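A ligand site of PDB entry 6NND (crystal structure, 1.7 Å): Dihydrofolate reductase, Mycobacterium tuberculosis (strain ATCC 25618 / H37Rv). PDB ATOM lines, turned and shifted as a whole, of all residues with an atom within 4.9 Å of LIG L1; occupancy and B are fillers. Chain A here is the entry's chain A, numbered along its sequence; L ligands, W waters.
OD2 of Asp 27 sits at hydrogen-bond distance from N3 of LIG L1.
An oxygen (O14) of LG2 L2 sits at hydrogen-bond distance from the backbone NH of Ala 7 (2.9 Å).
The backbone carbonyl oxygen (O) of Ala 7 sits at hydrogen-bond distance from a nitrogen (N7) of LG2 L2 (2.8 Å).
The side-chain hydroxyl (OG1) of Thr 46 lies within hydrogen-bond range of an oxygen (O1) of LG2 L2 (2.7 Å).
N of Thr 46 sits at hydrogen-bond distance from O1 of LG2 L2 (3.1 Å).
An oxygen (O6) of LIG L1 lies within salt-bridge range of the guanidinium group (NH2) of Arg 60 (2.8 Å).
O of Trp 6 sits close to N2 of LIG L1 (3.4 Å).
Merely in contact with LIG L1: Ile 94, Phe 31, Gln 28, Arg 32, Ala 7, Thr 113, Leu 50, Ala 29, Val 54, Leu 57, Ile 5, Tyr 100, Pro 51 and Ile 20.
Hydrophobic or aromatic side chains that line LIG L1: Ile 5, Ala 7, Ile 20, Ala 29, Phe 31, Leu 50, Pro 51, Val 54 and Leu 57.
The nearest printed residue that does not touch LIG L1 is Pro 58 (4.3 Å).
Water W2 bridges O3 of LIG L1 and O of Pro 25.
Water W5 bridges O1 of LIG L1 (2.7 Å) and NE2 of Gln 28 (2.9 Å).
Water W9 lies within hydrogen-bond range of OG1 of Thr 113, N2 of LIG L1, O of Trp 6 and NE2 of His 30.
Water W3 lies within hydrogen-bond range of N6 of LIG L1 and O of Ser 49.
Water W7 lies within hydrogen-bond range of the side-chain hydroxyl of Ser 49 (2.6 Å), an oxygen (O13) of LG2 L2 (2.7 Å) and a nitrogen (N6) of LIG L1 (3.4 Å).
Water W1 bridges the side-chain carboxylate (OD2) of Asp 27 and an oxygen (O1) of LIG L1.
OH of Tyr 100 is in hydrogen-bond range of O of Ile 5, 2.5 Å away.
O of Trp 6 sits at hydrogen-bond distance from N of Thr 113 (2.9 Å).
The backbone carbonyl oxygen (O) of Ile 94 is in hydrogen-bond range of the side-chain hydroxyl (OH) of Tyr 100.
The guanidinium group (NH1) of Arg 60 sits at hydrogen-bond distance from the side-chain hydroxyl (OG1) of Thr 35.
The side-chain hydroxyl (OG1) of Thr 35 is in hydrogen-bond range of the backbone carbonyl oxygen (O) of Phe 31, 2.8 Å away.
The backbone carbonyl oxygen (O) of Pro 58 is in hydrogen-bond range of the guanidinium group (NE) of Arg 60 (2.8 Å).
OG1 of Thr 113 lies within hydrogen-bond range of OD1 of Asp 27 (2.6 Å).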
ATOM      1  N   ILE A   5     -12.938 -19.282  12.269  1.00  0.00           N
ATOM      2  CA  ILE A   5     -11.723 -20.080  12.135  1.00  0.00           C
ATOM      3  C   ILE A   5     -10.617 -19.170  11.618  1.00  0.00           C
ATOM      4  O   ILE A   5     -10.853 -18.371  10.697  1.00  0.00           O
ATOM      5  CB  ILE A   5     -11.965 -21.306  11.230  1.00  0.00           C
ATOM      6  CG1 ILE A   5     -10.700 -22.142  11.062  1.00  0.00           C
ATOM      7  CG2 ILE A   5     -12.578 -20.881   9.861  1.00  0.00           C
ATOM      8  CD1 ILE A   5     -11.018 -23.597  10.718  1.00  0.00           C
ATOM      9  N   TRP A   6      -9.436 -19.216  12.255  1.00  0.00           N
ATOM     10  CA  TRP A   6      -8.320 -18.397  11.778  1.00  0.00           C
ATOM     11  C   TRP A   6      -7.009 -18.989  12.264  1.00  0.00           C
ATOM     12  O   TRP A   6      -6.984 -19.830  13.167  1.00  0.00           O
ATOM     13  CB  TRP A   6      -8.436 -16.930  12.241  1.00  0.00           C
ATOM     14  CG  TRP A   6      -8.141 -16.672  13.707  1.00  0.00           C
ATOM     15  CD1 TRP A   6      -6.907 -16.511  14.290  1.00  0.00           C
ATOM     16  CD2 TRP A   6      -9.109 -16.457  14.764  1.00  0.00           C
ATOM     17  NE1 TRP A   6      -7.057 -16.256  15.642  1.00  0.00           N
ATOM     18  CE2 TRP A   6      -8.393 -16.203  15.946  1.00  0.00           C
ATOM     19  CE3 TRP A   6     -10.508 -16.483  14.814  1.00  0.00           C
ATOM     20  CZ2 TRP A   6      -9.025 -15.980  17.186  1.00  0.00           C
ATOM     21  CZ3 TRP A   6     -11.140 -16.249  16.019  1.00  0.00           C
ATOM     22  CH2 TRP A   6     -10.400 -15.994  17.199  1.00  0.00           C
ATOM     23  N   ALA A   7      -5.924 -18.549  11.634  1.00  0.00           N
ATOM     24  CA  ALA A   7      -4.562 -18.837  12.089  1.00  0.00           C
ATOM     25  C   ALA A   7      -3.881 -17.515  12.413  1.00  0.00           C
ATOM     26  O   ALA A   7      -4.050 -16.532  11.696  1.00  0.00           O
ATOM     27  CB  ALA A   7      -3.761 -19.609  11.009  1.00  0.00           C
ATOM     28  N   ILE A  20      -1.176 -13.445   3.811  1.00  0.00           N
ATOM     29  CA  ILE A  20      -0.762 -14.067   5.071  1.00  0.00           C
ATOM     30  C   ILE A  20       0.728 -14.362   5.012  1.00  0.00           C
ATOM     31  O   ILE A  20       1.195 -14.936   4.019  1.00  0.00           O
ATOM     32  CB  ILE A  20      -1.544 -15.364   5.347  1.00  0.00           C
ATOM     33  CG1 ILE A  20      -3.052 -15.116   5.342  1.00  0.00           C
ATOM     34  CG2 ILE A  20      -1.100 -15.988   6.672  1.00  0.00           C
ATOM     35  CD1 ILE A  20      -3.866 -16.403   5.439  1.00  0.00           C
ATOM     36  N   PRO A  25       0.580 -26.279   5.414  1.00  0.00           N
ATOM     37  CA  PRO A  25      -0.343 -27.176   4.698  1.00  0.00           C
ATOM     38  C   PRO A  25      -1.267 -27.929   5.635  1.00  0.00           C
ATOM     39  O   PRO A  25      -2.441 -28.104   5.319  1.00  0.00           O
ATOM     40  CB  PRO A  25       0.619 -28.127   3.965  1.00  0.00           C
ATOM     41  CG  PRO A  25       1.855 -27.313   3.744  1.00  0.00           C
ATOM     42  CD  PRO A  25       1.979 -26.441   4.975  1.00  0.00           C
ATOM     43  N   ASP A  27      -2.465 -26.837   8.421  1.00  0.00           N
ATOM     44  CA  ASP A  27      -3.491 -25.911   8.894  1.00  0.00           C
ATOM     45  C   ASP A  27      -4.559 -25.694   7.832  1.00  0.00           C
ATOM     46  O   ASP A  27      -5.758 -25.657   8.133  1.00  0.00           O
ATOM     47  CB  ASP A  27      -2.816 -24.597   9.292  1.00  0.00           C
ATOM     48  CG  ASP A  27      -3.791 -23.551   9.745  1.00  0.00           C
ATOM     49  OD1 ASP A  27      -4.655 -23.885  10.574  1.00  0.00           O
ATOM     50  OD2 ASP A  27      -3.664 -22.415   9.283  1.00  0.00           O
ATOM     51  N   GLN A  28      -4.149 -25.628   6.562  1.00  0.00           N
ATOM     52  CA  GLN A  28      -5.127 -25.496   5.473  1.00  0.00           C
ATOM     53  C   GLN A  28      -5.969 -26.767   5.343  1.00  0.00           C
ATOM     54  O   GLN A  28      -7.163 -26.692   5.030  1.00  0.00           O
ATOM     55  CB  GLN A  28      -4.385 -25.192   4.165  1.00  0.00           C
ATOM     56  CG  GLN A  28      -3.827 -23.774   4.132  1.00  0.00           C
ATOM     57  CD  GLN A  28      -3.357 -23.372   2.764  1.00  0.00           C
ATOM     58  OE1 GLN A  28      -2.827 -24.192   2.008  1.00  0.00           O
ATOM     59  NE2 GLN A  28      -3.547 -22.110   2.423  1.00  0.00           N
ATOM     60  N   ALA A  29      -5.376 -27.927   5.579  1.00  0.00           N
ATOM     61  CA  ALA A  29      -6.159 -29.161   5.562  1.00  0.00           C
ATOM     62  C   ALA A  29      -7.166 -29.181   6.703  1.00  0.00           C
ATOM     63  O   ALA A  29      -8.333 -29.570   6.525  1.00  0.00           O
ATOM     64  CB  ALA A  29      -5.213 -30.370   5.648  1.00  0.00           C
ATOM     65  N   HIS A  30      -6.745 -28.737   7.884  1.00  0.00           N
ATOM     66  CA  HIS A  30      -7.659 -28.606   9.013  1.00  0.00           C
ATOM     67  C   HIS A  30      -8.776 -27.617   8.670  1.00  0.00           C
ATOM     68  O   HIS A  30      -9.959 -27.888   8.920  1.00  0.00           O
ATOM     69  CB  HIS A  30      -6.849 -28.152  10.234  1.00  0.00           C
ATOM     70  CG  HIS A  30      -7.672 -27.613  11.355  1.00  0.00           C
ATOM     71  ND1 HIS A  30      -8.421 -28.418  12.181  1.00  0.00           N
ATOM     72  CD2 HIS A  30      -7.806 -26.350  11.818  1.00  0.00           C
ATOM     73  CE1 HIS A  30      -9.011 -27.673  13.092  1.00  0.00           C
ATOM     74  NE2 HIS A  30      -8.654 -26.410  12.902  1.00  0.00           N
ATOM     75  N   PHE A  31      -8.415 -26.491   8.048  1.00  0.00           N
ATOM     76  CA  PHE A  31      -9.422 -25.521   7.625  1.00  0.00           C
ATOM     77  C   PHE A  31     -10.436 -26.168   6.688  1.00  0.00           C
ATOM     78  O   PHE A  31     -11.641 -25.984   6.847  1.00  0.00           O
ATOM     79  CB  PHE A  31      -8.729 -24.331   6.942  1.00  0.00           C
ATOM     80  CG  PHE A  31      -9.663 -23.420   6.201  1.00  0.00           C
ATOM     81  CD1 PHE A  31     -10.210 -22.315   6.828  1.00  0.00           C
ATOM     82  CD2 PHE A  31     -10.010 -23.688   4.890  1.00  0.00           C
ATOM     83  CE1 PHE A  31     -11.096 -21.467   6.149  1.00  0.00           C
ATOM     84  CE2 PHE A  31     -10.888 -22.859   4.197  1.00  0.00           C
ATOM     85  CZ  PHE A  31     -11.422 -21.742   4.838  1.00  0.00           C
ATOM     86  N   ARG A  32      -9.943 -26.945   5.707  1.00  0.00           N
ATOM     87  CA  ARG A  32     -10.850 -27.597   4.769  1.00  0.00           C
ATOM     88  C   ARG A  32     -11.783 -28.571   5.486  1.00  0.00           C
ATOM     89  O   ARG A  32     -12.978 -28.605   5.210  1.00  0.00           O
ATOM     90  CB  ARG A  32     -10.057 -28.333   3.689  1.00  0.00           C
ATOM     91  CG  ARG A  32     -10.947 -29.056   2.682  1.00  0.00           C
ATOM     92  CD  ARG A  32     -10.155 -29.963   1.727  1.00  0.00           C
ATOM     93  NE  ARG A  32     -11.038 -30.977   1.141  1.00  0.00           N
ATOM     94  CZ  ARG A  32     -11.321 -32.145   1.715  1.00  0.00           C
ATOM     95  NH1 ARG A  32     -10.787 -32.462   2.883  1.00  0.00           N
ATOM     96  NH2 ARG A  32     -12.144 -32.997   1.111  1.00  0.00           N
ATOM     97  N   THR A  35     -14.541 -26.663   7.516  1.00  0.00           N
ATOM     98  CA  THR A  35     -15.504 -25.840   6.778  1.00  0.00           C
ATOM     99  C   THR A  35     -16.275 -26.619   5.726  1.00  0.00           C
ATOM    100  O   THR A  35     -17.358 -26.153   5.338  1.00  0.00           O
ATOM    101  CB  THR A  35     -14.825 -24.647   6.091  1.00  0.00           C
ATOM    102  OG1 THR A  35     -13.769 -25.096   5.233  1.00  0.00           O
ATOM    103  CG2 THR A  35     -14.266 -23.659   7.118  1.00  0.00           C
ATOM    104  N   THR A  46     -10.777 -10.664   1.928  1.00  0.00           N
ATOM    105  CA  THR A  46     -10.380 -12.064   2.060  1.00  0.00           C
ATOM    106  C   THR A  46     -10.769 -12.871   0.816  1.00  0.00           C
ATOM    107  O   THR A  46     -10.004 -13.715   0.348  1.00  0.00           O
ATOM    108  CB  THR A  46     -10.964 -12.648   3.352  1.00  0.00           C
ATOM    109  OG1 THR A  46     -10.301 -12.039   4.485  1.00  0.00           O
ATOM    110  CG2 THR A  46     -10.774 -14.153   3.414  1.00  0.00           C
ATOM    111  N   SER A  49      -8.145 -12.348  -1.537  1.00  0.00           N
ATOM    112  CA  SER A  49      -6.921 -13.026  -1.142  1.00  0.00           C
ATOM    113  C   SER A  49      -6.936 -14.528  -1.438  1.00  0.00           C
ATOM    114  O   SER A  49      -5.884 -15.174  -1.308  1.00  0.00           O
ATOM    115  CB  SER A  49      -6.648 -12.832   0.345  1.00  0.00           C
ATOM    116  OG  SER A  49      -7.383 -13.758   1.121  1.00  0.00           O
ATOM    117  N   LEU A  50      -8.098 -15.102  -1.744  1.00  0.00           N
ATOM    118  CA  LEU A  50      -8.132 -16.533  -2.050  1.00  0.00           C
ATOM    119  C   LEU A  50      -7.407 -16.799  -3.358  1.00  0.00           C
ATOM    120  O   LEU A  50      -7.641 -16.085  -4.338  1.00  0.00           O
ATOM    121  CB  LEU A  50      -9.584 -17.031  -2.153  1.00  0.00           C
ATOM    122  CG  LEU A  50     -10.372 -17.010  -0.849  1.00  0.00           C
ATOM    123  CD1 LEU A  50     -11.787 -17.518  -1.118  1.00  0.00           C
ATOM    124  CD2 LEU A  50      -9.670 -17.850   0.249  1.00  0.00           C
ATOM    125  N   PRO A  51      -6.551 -17.816  -3.431  1.00  0.00           N
ATOM    126  CA  PRO A  51      -5.948 -18.176  -4.718  1.00  0.00           C
ATOM    127  C   PRO A  51      -7.037 -18.480  -5.738  1.00  0.00           C
ATOM    128  O   PRO A  51      -8.050 -19.109  -5.421  1.00  0.00           O
ATOM    129  CB  PRO A  51      -5.119 -19.434  -4.391  1.00  0.00           C
ATOM    130  CG  PRO A  51      -4.851 -19.354  -2.922  1.00  0.00           C
ATOM    131  CD  PRO A  51      -6.053 -18.659  -2.325  1.00  0.00           C
ATOM    132  N   VAL A  54      -8.957 -21.714  -5.897  1.00  0.00           N
ATOM    133  CA  VAL A  54      -9.923 -22.133  -4.888  1.00  0.00           C
ATOM    134  C   VAL A  54     -10.935 -21.014  -4.664  1.00  0.00           C
ATOM    135  O   VAL A  54     -11.330 -20.729  -3.526  1.00  0.00           O
ATOM    136  CB  VAL A  54      -9.228 -22.514  -3.570  1.00  0.00           C
ATOM    137  CG1 VAL A  54      -8.491 -23.853  -3.709  1.00  0.00           C
ATOM    138  CG2 VAL A  54      -8.289 -21.422  -3.127  1.00  0.00           C
ATOM    139  N   LEU A  57     -14.200 -21.625  -2.846  1.00  0.00           N
ATOM    140  CA  LEU A  57     -13.741 -22.834  -2.177  1.00  0.00           C
ATOM    141  C   LEU A  57     -14.772 -23.949  -2.407  1.00  0.00           C
ATOM    142  O   LEU A  57     -15.973 -23.740  -2.162  1.00  0.00           O
ATOM    143  CB  LEU A  57     -13.520 -22.554  -0.685  1.00  0.00           C
ATOM    144  CG  LEU A  57     -12.304 -21.678  -0.377  1.00  0.00           C
ATOM    145  CD1 LEU A  57     -12.349 -21.051   1.010  1.00  0.00           C
ATOM    146  CD2 LEU A  57     -11.044 -22.511  -0.507  1.00  0.00           C
ATOM    147  N   PRO A  58     -14.348 -25.121  -2.890  1.00  0.00           N
ATOM    148  CA  PRO A  58     -15.310 -26.156  -3.316  1.00  0.00           C
ATOM    149  C   PRO A  58     -16.114 -26.780  -2.186  1.00  0.00           C
ATOM    150  O   PRO A  58     -15.628 -26.952  -1.066  1.00  0.00           O
ATOM    151  CB  PRO A  58     -14.434 -27.214  -3.989  1.00  0.00           C
ATOM    152  CG  PRO A  58     -13.081 -26.629  -4.107  1.00  0.00           C
ATOM    153  CD  PRO A  58     -12.957 -25.513  -3.158  1.00  0.00           C
ATOM    154  N   ARG A  60     -18.664 -25.713  -0.598  1.00  0.00           N
ATOM    155  CA  ARG A  60     -19.110 -24.793   0.432  1.00  0.00           C
ATOM    156  C   ARG A  60     -19.901 -23.669  -0.208  1.00  0.00           C
ATOM    157  O   ARG A  60     -19.615 -23.237  -1.331  1.00  0.00           O
ATOM    158  CB  ARG A  60     -17.910 -24.214   1.220  1.00  0.00           C
ATOM    159  CG  ARG A  60     -17.310 -25.200   2.231  1.00  0.00           C
ATOM    160  CD  ARG A  60     -15.804 -24.964   2.440  1.00  0.00           C
ATOM    161  NE  ARG A  60     -15.043 -25.535   1.323  1.00  0.00           N
ATOM    162  CZ  ARG A  60     -13.729 -25.668   1.338  1.00  0.00           C
ATOM    163  NH1 ARG A  60     -13.022 -25.272   2.404  1.00  0.00           N
ATOM    164  NH2 ARG A  60     -13.097 -26.204   0.297  1.00  0.00           N
ATOM    165  N   ILE A  94     -14.664 -16.960   7.891  1.00  0.00           N
ATOM    166  CA  ILE A  94     -13.274 -17.249   7.565  1.00  0.00           C
ATOM    167  C   ILE A  94     -12.450 -15.973   7.372  1.00  0.00           C
ATOM    168  O   ILE A  94     -11.406 -16.004   6.743  1.00  0.00           O
ATOM    169  CB  ILE A  94     -13.165 -18.185   6.354  1.00  0.00           C
ATOM    170  CG1 ILE A  94     -13.729 -17.530   5.102  1.00  0.00           C
ATOM    171  CG2 ILE A  94     -13.899 -19.478   6.626  1.00  0.00           C
ATOM    172  CD1 ILE A  94     -13.188 -18.241   3.823  1.00  0.00           C
ATOM    173  N   TYR A 100     -14.102 -10.842  11.226  1.00  0.00           N
ATOM    174  CA  TYR A 100     -14.049 -11.552  12.510  1.00  0.00           C
ATOM    175  C   TYR A 100     -14.648 -10.697  13.619  1.00  0.00           C
ATOM    176  O   TYR A 100     -15.422 -11.185  14.441  1.00  0.00           O
ATOM    177  CB  TYR A 100     -12.600 -11.929  12.883  1.00  0.00           C
ATOM    178  CG  TYR A 100     -11.964 -13.046  12.073  1.00  0.00           C
ATOM    179  CD1 TYR A 100     -12.665 -14.227  11.787  1.00  0.00           C
ATOM    180  CD2 TYR A 100     -10.648 -12.925  11.598  1.00  0.00           C
ATOM    181  CE1 TYR A 100     -12.077 -15.253  11.037  1.00  0.00           C
ATOM    182  CE2 TYR A 100     -10.069 -13.938  10.840  1.00  0.00           C
ATOM    183  CZ  TYR A 100     -10.774 -15.100  10.577  1.00  0.00           C
ATOM    184  OH  TYR A 100     -10.203 -16.093   9.809  1.00  0.00           O
ATOM    185  N   THR A 113      -5.687 -21.594  15.077  1.00  0.00           N
ATOM    186  CA  THR A 113      -4.350 -22.156  14.950  1.00  0.00           C
ATOM    187  C   THR A 113      -3.377 -21.088  15.389  1.00  0.00           C
ATOM    188  O   THR A 113      -3.362 -19.986  14.831  1.00  0.00           O
ATOM    189  CB  THR A 113      -4.059 -22.577  13.508  1.00  0.00           C
ATOM    190  OG1 THR A 113      -5.040 -23.528  13.082  1.00  0.00           O
ATOM    191  CG2 THR A 113      -2.624 -23.170  13.390  1.00  0.00           C
HETATM  192  N1  LIG L   1      -7.976 -20.397   8.914  1.00  0.00           N
HETATM  193  C1  LIG L   1      -6.874 -21.070   9.226  1.00  0.00           C
HETATM  194  N2  LIG L   1      -6.795 -21.859  10.391  1.00  0.00           N
HETATM  195  N3  LIG L   1      -5.762 -21.052   8.406  1.00  0.00           N
HETATM  196  C2  LIG L   1      -5.719 -20.382   7.315  1.00  0.00           C
HETATM  197  O1  LIG L   1      -4.726 -20.402   6.667  1.00  0.00           O
HETATM  198  C3  LIG L   1      -6.853 -19.682   6.983  1.00  0.00           C
HETATM  199  N4  LIG L   1      -6.826 -18.953   5.745  1.00  0.00           N
HETATM  200  C4  LIG L   1      -7.920 -18.234   5.378  1.00  0.00           C
HETATM  201  C5  LIG L   1      -9.154 -18.258   6.253  1.00  0.00           C
HETATM  202  N5  LIG L   1      -9.147 -18.968   7.414  1.00  0.00           N
HETATM  203  C6  LIG L   1      -7.978 -19.697   7.799  1.00  0.00           C
HETATM  204  C7  LIG L   1      -7.901 -17.450   4.092  1.00  0.00           C
HETATM  205  N6  LIG L   1      -7.112 -18.065   3.079  1.00  0.00           N
HETATM  206  C8  LIG L   1      -7.276 -21.825   1.190  1.00  0.00           C
HETATM  207  C9  LIG L   1      -8.186 -21.528   2.182  1.00  0.00           C
HETATM  208  C10 LIG L   1      -8.158 -20.315   2.805  1.00  0.00           C
HETATM  209  C11 LIG L   1      -7.235 -19.378   2.486  1.00  0.00           C
HETATM  210  C12 LIG L   1      -6.331 -19.701   1.512  1.00  0.00           C
HETATM  211  C13 LIG L   1      -6.349 -20.901   0.871  1.00  0.00           C
HETATM  212  C14 LIG L   1      -7.289 -23.140   0.503  1.00  0.00           C
HETATM  213  O2  LIG L   1      -6.680 -23.354  -0.416  1.00  0.00           O
HETATM  214  N7  LIG L   1      -8.110 -24.141   1.049  1.00  0.00           N
HETATM  215  C15 LIG L   1      -8.292 -25.461   0.546  1.00  0.00           C
HETATM  216  C16 LIG L   1      -7.262 -26.296   1.283  1.00  0.00           C
HETATM  217  C17 LIG L   1      -7.254 -27.723   0.931  1.00  0.00           C
HETATM  218  C18 LIG L   1      -6.105 -28.476   1.605  1.00  0.00           C
HETATM  219  O3  LIG L   1      -5.104 -27.849   1.797  1.00  0.00           O
HETATM  220  O4  LIG L   1      -6.229 -29.677   1.936  1.00  0.00           O
HETATM  221  C19 LIG L   1      -9.746 -25.844   0.877  1.00  0.00           C
HETATM  222  O5  LIG L   1     -10.240 -25.360   1.907  1.00  0.00           O
HETATM  223  O6  LIG L   1     -10.325 -26.608   0.084  1.00  0.00           O
HETATM  224  P1  LG2 L   2     -11.773  -8.327   5.491  1.00  0.00           P
HETATM  225  O1  LG2 L   2     -11.337  -9.599   4.808  1.00  0.00           O
HETATM  226  O2  LG2 L   2     -12.348  -8.350   6.857  1.00  0.00           O
HETATM  227  O3  LG2 L   2     -12.787  -7.620   4.362  1.00  0.00           O
HETATM  228  C1  LG2 L   2     -12.972  -6.249   4.656  1.00  0.00           C
HETATM  229  C2  LG2 L   2     -14.074  -5.800   3.663  1.00  0.00           C
HETATM  230  O4  LG2 L   2     -15.281  -6.499   4.002  1.00  0.00           O
HETATM  231  C3  LG2 L   2     -14.412  -4.275   3.678  1.00  0.00           C
HETATM  232  O5  LG2 L   2     -13.483  -3.581   2.838  1.00  0.00           O
HETATM  233  C4  LG2 L   2     -15.828  -4.360   2.991  1.00  0.00           C
HETATM  234  O6  LG2 L   2     -15.814  -4.757   1.706  1.00  0.00           O
HETATM  235  C5  LG2 L   2     -16.404  -5.603   3.743  1.00  0.00           C
HETATM  236  N1  LG2 L   2     -17.041  -5.247   5.015  1.00  0.00           N
HETATM  237  C6  LG2 L   2     -16.456  -5.066   6.277  1.00  0.00           C
HETATM  238  N2  LG2 L   2     -17.376  -4.718   7.245  1.00  0.00           N
HETATM  239  C7  LG2 L   2     -18.595  -4.666   6.548  1.00  0.00           C
HETATM  240  C8  LG2 L   2     -19.904  -4.369   6.956  1.00  0.00           C
HETATM  241  N3  LG2 L   2     -20.207  -4.040   8.267  1.00  0.00           N
HETATM  242  N4  LG2 L   2     -20.928  -4.392   6.060  1.00  0.00           N
HETATM  243  C9  LG2 L   2     -20.592  -4.717   4.763  1.00  0.00           C
HETATM  244  N5  LG2 L   2     -19.403  -5.026   4.217  1.00  0.00           N
HETATM  245  C10 LG2 L   2     -18.398  -4.984   5.155  1.00  0.00           C
HETATM  246  O7  LG2 L   2     -10.461  -7.273   5.382  1.00  0.00           O
HETATM  247  P2  LG2 L   2      -9.263  -7.282   6.474  1.00  0.00           P
HETATM  248  O8  LG2 L   2      -8.281  -6.344   5.872  1.00  0.00           O
HETATM  249  O9  LG2 L   2      -9.669  -7.118   7.920  1.00  0.00           O
HETATM  250  O10 LG2 L   2      -8.594  -8.843   6.502  1.00  0.00           O
HETATM  251  C11 LG2 L   2      -7.934  -9.179   5.284  1.00  0.00           C
HETATM  252  C12 LG2 L   2      -6.587  -9.768   5.716  1.00  0.00           C
HETATM  253  O11 LG2 L   2      -6.801 -10.903   6.579  1.00  0.00           O
HETATM  254  C13 LG2 L   2      -5.738 -10.273   4.485  1.00  0.00           C
HETATM  255  O12 LG2 L   2      -4.411 -10.044   4.860  1.00  0.00           O
HETATM  256  C14 LG2 L   2      -6.051 -11.765   4.521  1.00  0.00           C
HETATM  257  O13 LG2 L   2      -5.047 -12.559   3.917  1.00  0.00           O
HETATM  258  C15 LG2 L   2      -6.043 -11.998   6.077  1.00  0.00           C
HETATM  259  N6  LG2 L   2      -6.703 -13.266   6.478  1.00  0.00           N
HETATM  260  C16 LG2 L   2      -6.050 -14.156   7.323  1.00  0.00           C
HETATM  261  C17 LG2 L   2      -6.682 -15.262   7.814  1.00  0.00           C
HETATM  262  C18 LG2 L   2      -5.967 -16.156   8.717  1.00  0.00           C
HETATM  263  O14 LG2 L   2      -6.497 -17.168   9.198  1.00  0.00           O
HETATM  264  N7  LG2 L   2      -4.638 -15.854   9.047  1.00  0.00           N
HETATM  265  C19 LG2 L   2      -8.070 -15.570   7.471  1.00  0.00           C
HETATM  266  C20 LG2 L   2      -8.677 -14.599   6.511  1.00  0.00           C
HETATM  267  C21 LG2 L   2      -8.025 -13.528   6.071  1.00  0.00           C
HETATM  268  P3  LG2 L   2     -15.836  -3.515   0.465  1.00  0.00           P
HETATM  269  O15 LG2 L   2     -17.087  -2.801   0.892  1.00  0.00           O
HETATM  270  O16 LG2 L   2     -14.511  -2.777   0.663  1.00  0.00           O
HETATM  271  O17 LG2 L   2     -15.951  -4.399  -0.758  1.00  0.00           O
HETATM  272  O   HOH W   1      -1.635 -21.698   7.239  1.00  0.00           O
HETATM  273  O   HOH W   2      -3.121 -29.179   2.756  1.00  0.00           O
HETATM  274  O   HOH W   3      -4.768 -16.449   1.541  1.00  0.00           O
HETATM  275  O   HOH W   4      -7.823 -30.178  -1.154  1.00  0.00           O
HETATM  276  O   HOH W   5      -4.140 -19.857   4.121  1.00  0.00           O
HETATM  277  O   HOH W   6      -9.658 -27.780  -1.925  1.00  0.00           O
HETATM  278  O   HOH W   7      -6.154 -14.852   3.155  1.00  0.00           O
HETATM  279  O   HOH W   8      -7.112 -31.817   2.829  1.00  0.00           O
HETATM  280  O   HOH W   9      -7.806 -23.081  12.908  1.00  0.00           O
